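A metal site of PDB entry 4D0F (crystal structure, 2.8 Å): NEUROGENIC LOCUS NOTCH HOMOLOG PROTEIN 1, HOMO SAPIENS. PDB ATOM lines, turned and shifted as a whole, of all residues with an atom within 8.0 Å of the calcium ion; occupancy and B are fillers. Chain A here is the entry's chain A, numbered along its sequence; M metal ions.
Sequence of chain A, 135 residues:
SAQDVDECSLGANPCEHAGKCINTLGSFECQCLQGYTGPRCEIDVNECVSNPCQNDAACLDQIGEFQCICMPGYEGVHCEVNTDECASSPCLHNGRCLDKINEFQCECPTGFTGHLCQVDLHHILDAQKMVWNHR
OD1 of Asp 44 is bound to the calcium ion (2.1 Å). The calcium ion is bound by the backbone carbonyl oxygen (O) of Gln 62 (2.2 Å). The calcium ion is bound by OE1 of Glu 47 (2.4 Å). The calcium ion is bound by O of Val 45, at 2.4 Å. OD1 of Asp 61 is bound to the calcium ion (2.6 Å).
N of Asp 61 is in hydrogen-bond range of SG of Cys 48, at 3.6 Å. OD1 of Asn 46 sits close to OD2 of Asp 61, at 3.3 Å. The backbone NH (N) of Val 45 sits at hydrogen-bond distance from the backbone carbonyl oxygen (O) of Gly 35.
Within 4 Å of the calcium ion: Asp 44, Val 45, Glu 47, Asp 61 and Gln 62.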
ATOM      1  N   GLN A  34      -3.790 -20.769  32.477  1.00  0.00           N
ATOM      2  CA  GLN A  34      -4.103 -19.769  31.465  1.00  0.00           C
ATOM      3  C   GLN A  34      -3.415 -20.080  30.154  1.00  0.00           C
ATOM      4  O   GLN A  34      -2.213 -20.395  30.116  1.00  0.00           O
ATOM      5  CB  GLN A  34      -3.737 -18.372  31.934  1.00  0.00           C
ATOM      6  CG  GLN A  34      -4.252 -17.261  31.028  1.00  0.00           C
ATOM      7  CD  GLN A  34      -4.263 -15.947  31.740  1.00  0.00           C
ATOM      8  OE1 GLN A  34      -4.589 -15.865  32.937  1.00  0.00           O
ATOM      9  NE2 GLN A  34      -3.928 -14.902  30.990  1.00  0.00           N
ATOM     10  N   GLY A  35      -4.214 -20.036  29.092  1.00  0.00           N
ATOM     11  CA  GLY A  35      -3.759 -20.287  27.737  1.00  0.00           C
ATOM     12  C   GLY A  35      -4.007 -21.678  27.249  1.00  0.00           C
ATOM     13  O   GLY A  35      -3.687 -21.978  26.099  1.00  0.00           O
ATOM     14  N   TYR A  36      -4.584 -22.554  28.125  1.00  0.00           N
ATOM     15  CA  TYR A  36      -4.886 -23.931  27.741  1.00  0.00           C
ATOM     16  C   TYR A  36      -6.354 -24.231  27.877  1.00  0.00           C
ATOM     17  O   TYR A  36      -7.006 -23.696  28.784  1.00  0.00           O
ATOM     18  CB  TYR A  36      -4.034 -24.909  28.520  1.00  0.00           C
ATOM     19  CG  TYR A  36      -2.555 -24.726  28.308  1.00  0.00           C
ATOM     20  CD1 TYR A  36      -1.938 -25.178  27.132  1.00  0.00           C
ATOM     21  CD2 TYR A  36      -1.768 -24.087  29.260  1.00  0.00           C
ATOM     22  CE1 TYR A  36      -0.570 -25.007  26.928  1.00  0.00           C
ATOM     23  CE2 TYR A  36      -0.402 -23.892  29.057  1.00  0.00           C
ATOM     24  CZ  TYR A  36       0.198 -24.362  27.883  1.00  0.00           C
ATOM     25  OH  TYR A  36       1.553 -24.210  27.703  1.00  0.00           O
ATOM     26  N   ILE A  43      -5.205 -28.418  24.478  1.00  0.00           N
ATOM     27  CA  ILE A  43      -5.087 -27.363  23.496  1.00  0.00           C
ATOM     28  C   ILE A  43      -4.445 -26.091  23.956  1.00  0.00           C
ATOM     29  O   ILE A  43      -4.858 -25.498  24.954  1.00  0.00           O
ATOM     30  CB  ILE A  43      -6.458 -27.093  22.780  1.00  0.00           C
ATOM     31  CG1 ILE A  43      -7.302 -28.378  22.495  1.00  0.00           C
ATOM     32  CG2 ILE A  43      -6.315 -26.169  21.574  1.00  0.00           C
ATOM     33  CD1 ILE A  43      -6.702 -29.524  21.605  1.00  0.00           C
ATOM     34  N   ASP A  44      -3.495 -25.621  23.161  1.00  0.00           N
ATOM     35  CA  ASP A  44      -2.874 -24.339  23.335  1.00  0.00           C
ATOM     36  C   ASP A  44      -3.805 -23.367  22.550  1.00  0.00           C
ATOM     37  O   ASP A  44      -3.824 -23.344  21.313  1.00  0.00           O
ATOM     38  CB  ASP A  44      -1.448 -24.358  22.775  1.00  0.00           C
ATOM     39  CG  ASP A  44      -0.783 -23.012  22.618  1.00  0.00           C
ATOM     40  OD1 ASP A  44      -1.415 -21.984  22.964  1.00  0.00           O
ATOM     41  OD2 ASP A  44       0.378 -22.978  22.153  1.00  0.00           O
ATOM     42  N   VAL A  45      -4.588 -22.588  23.305  1.00  0.00           N
ATOM     43  CA  VAL A  45      -5.500 -21.581  22.761  1.00  0.00           C
ATOM     44  C   VAL A  45      -4.781 -20.693  21.742  1.00  0.00           C
ATOM     45  O   VAL A  45      -3.627 -20.295  21.972  1.00  0.00           O
ATOM     46  CB  VAL A  45      -6.134 -20.698  23.879  1.00  0.00           C
ATOM     47  CG1 VAL A  45      -7.006 -19.577  23.327  1.00  0.00           C
ATOM     48  CG2 VAL A  45      -6.933 -21.541  24.835  1.00  0.00           C
ATOM     49  N   ASN A  46      -5.465 -20.364  20.636  1.00  0.00           N
ATOM     50  CA  ASN A  46      -4.962 -19.429  19.641  1.00  0.00           C
ATOM     51  C   ASN A  46      -5.421 -18.012  20.071  1.00  0.00           C
ATOM     52  O   ASN A  46      -6.541 -17.586  19.777  1.00  0.00           O
ATOM     53  CB  ASN A  46      -5.464 -19.752  18.229  1.00  0.00           C
ATOM     54  CG  ASN A  46      -5.019 -18.746  17.186  1.00  0.00           C
ATOM     55  OD1 ASN A  46      -4.169 -17.877  17.422  1.00  0.00           O
ATOM     56  ND2 ASN A  46      -5.592 -18.856  15.996  1.00  0.00           N
ATOM     57  N   GLU A  47      -4.529 -17.283  20.751  1.00  0.00           N
ATOM     58  CA  GLU A  47      -4.832 -15.946  21.260  1.00  0.00           C
ATOM     59  C   GLU A  47      -4.999 -14.911  20.149  1.00  0.00           C
ATOM     60  O   GLU A  47      -5.453 -13.809  20.437  1.00  0.00           O
ATOM     61  CB  GLU A  47      -3.808 -15.501  22.317  1.00  0.00           C
ATOM     62  CG  GLU A  47      -3.953 -16.191  23.667  1.00  0.00           C
ATOM     63  CD  GLU A  47      -3.316 -17.560  23.767  1.00  0.00           C
ATOM     64  OE1 GLU A  47      -2.413 -17.852  22.953  1.00  0.00           O
ATOM     65  OE2 GLU A  47      -3.786 -18.381  24.582  1.00  0.00           O
ATOM     66  N   CYS A  48      -4.683 -15.294  18.889  1.00  0.00           N
ATOM     67  CA  CYS A  48      -4.799 -14.445  17.700  1.00  0.00           C
ATOM     68  C   CYS A  48      -6.098 -14.590  16.948  1.00  0.00           C
ATOM     69  O   CYS A  48      -6.363 -13.826  16.020  1.00  0.00           O
ATOM     70  CB  CYS A  48      -3.609 -14.690  16.769  1.00  0.00           C
ATOM     71  SG  CYS A  48      -2.037 -14.127  17.431  1.00  0.00           S
ATOM     72  N   LEU A  60       1.335 -12.808  16.886  1.00  0.00           N
ATOM     73  CA  LEU A  60       2.083 -14.001  17.293  1.00  0.00           C
ATOM     74  C   LEU A  60       1.325 -14.754  18.366  1.00  0.00           C
ATOM     75  O   LEU A  60       1.073 -14.228  19.446  1.00  0.00           O
ATOM     76  CB  LEU A  60       3.494 -13.658  17.777  1.00  0.00           C
ATOM     77  CG  LEU A  60       4.410 -12.913  16.829  1.00  0.00           C
ATOM     78  CD1 LEU A  60       5.696 -12.667  17.480  1.00  0.00           C
ATOM     79  CD2 LEU A  60       4.626 -13.676  15.515  1.00  0.00           C
ATOM     80  N   ASP A  61       0.946 -15.993  18.069  1.00  0.00           N
ATOM     81  CA  ASP A  61       0.188 -16.827  18.996  1.00  0.00           C
ATOM     82  C   ASP A  61       1.179 -17.540  19.917  1.00  0.00           C
ATOM     83  O   ASP A  61       1.867 -18.463  19.492  1.00  0.00           O
ATOM     84  CB  ASP A  61      -0.683 -17.805  18.196  1.00  0.00           C
ATOM     85  CG  ASP A  61      -1.360 -18.904  19.002  1.00  0.00           C
ATOM     86  OD1 ASP A  61      -1.527 -18.720  20.226  1.00  0.00           O
ATOM     87  OD2 ASP A  61      -1.750 -19.918  18.407  1.00  0.00           O
ATOM     88  N   GLN A  62       1.248 -17.096  21.172  1.00  0.00           N
ATOM     89  CA  GLN A  62       2.219 -17.607  22.131  1.00  0.00           C
ATOM     90  C   GLN A  62       1.568 -18.333  23.283  1.00  0.00           C
ATOM     91  O   GLN A  62       0.373 -18.597  23.233  1.00  0.00           O
ATOM     92  CB  GLN A  62       3.098 -16.460  22.607  1.00  0.00           C
ATOM     93  CG  GLN A  62       3.749 -15.701  21.451  1.00  0.00           C
ATOM     94  CD  GLN A  62       4.402 -14.419  21.892  1.00  0.00           C
ATOM     95  OE1 GLN A  62       4.069 -13.833  22.936  1.00  0.00           O
ATOM     96  NE2 GLN A  62       5.357 -13.970  21.105  1.00  0.00           N
ATOM     97  N   ILE A  63       2.363 -18.704  24.303  1.00  0.00           N
ATOM     98  CA  ILE A  63       1.861 -19.435  25.455  1.00  0.00           C
ATOM     99  C   ILE A  63       1.092 -18.508  26.377  1.00  0.00           C
ATOM    100  O   ILE A  63       1.707 -17.620  26.980  1.00  0.00           O
ATOM    101  CB  ILE A  63       2.979 -20.271  26.173  1.00  0.00           C
ATOM    102  CG1 ILE A  63       3.769 -21.152  25.153  1.00  0.00           C
ATOM    103  CG2 ILE A  63       2.400 -21.098  27.326  1.00  0.00           C
ATOM    104  CD1 ILE A  63       5.095 -21.489  25.535  1.00  0.00           C
ATOM    105  N   GLY A  64      -0.239 -18.716  26.426  1.00  0.00           N
ATOM    106  CA  GLY A  64      -1.175 -17.944  27.245  1.00  0.00           C
ATOM    107  C   GLY A  64      -1.247 -16.461  26.942  1.00  0.00           C
ATOM    108  O   GLY A  64      -1.682 -15.678  27.787  1.00  0.00           O
ATOM    109  N   GLU A  65      -0.838 -16.052  25.717  1.00  0.00           N
ATOM    110  CA  GLU A  65      -0.769 -14.641  25.310  1.00  0.00           C
ATOM    111  C   GLU A  65      -0.519 -14.527  23.816  1.00  0.00           C
ATOM    112  O   GLU A  65      -0.131 -15.488  23.137  1.00  0.00           O
ATOM    113  CB  GLU A  65       0.456 -14.050  26.026  1.00  0.00           C
ATOM    114  CG  GLU A  65       0.441 -12.609  26.437  1.00  0.00           C
ATOM    115  CD  GLU A  65       1.802 -12.265  27.007  1.00  0.00           C
ATOM    116  OE1 GLU A  65       2.768 -13.023  26.736  1.00  0.00           O
ATOM    117  OE2 GLU A  65       1.905 -11.233  27.710  1.00  0.00           O
ATOM    118  N   PHE A  66      -0.716 -13.332  23.296  1.00  0.00           N
ATOM    119  CA  PHE A  66      -0.375 -12.965  21.941  1.00  0.00           C
ATOM    120  C   PHE A  66       0.601 -11.823  22.031  1.00  0.00           C
ATOM    121  O   PHE A  66       0.643 -11.132  23.041  1.00  0.00           O
ATOM    122  CB  PHE A  66      -1.597 -12.552  21.110  1.00  0.00           C
ATOM    123  CG  PHE A  66      -2.289 -11.312  21.618  1.00  0.00           C
ATOM    124  CD1 PHE A  66      -3.292 -11.397  22.573  1.00  0.00           C
ATOM    125  CD2 PHE A  66      -1.933 -10.060  21.145  1.00  0.00           C
ATOM    126  CE1 PHE A  66      -3.915 -10.257  23.060  1.00  0.00           C
ATOM    127  CE2 PHE A  66      -2.551  -8.912  21.650  1.00  0.00           C
ATOM    128  CZ  PHE A  66      -3.543  -9.021  22.589  1.00  0.00           C
HETATM  129 CA    CA M   1      -1.273 -19.923  22.515  1.00  0.00          CA
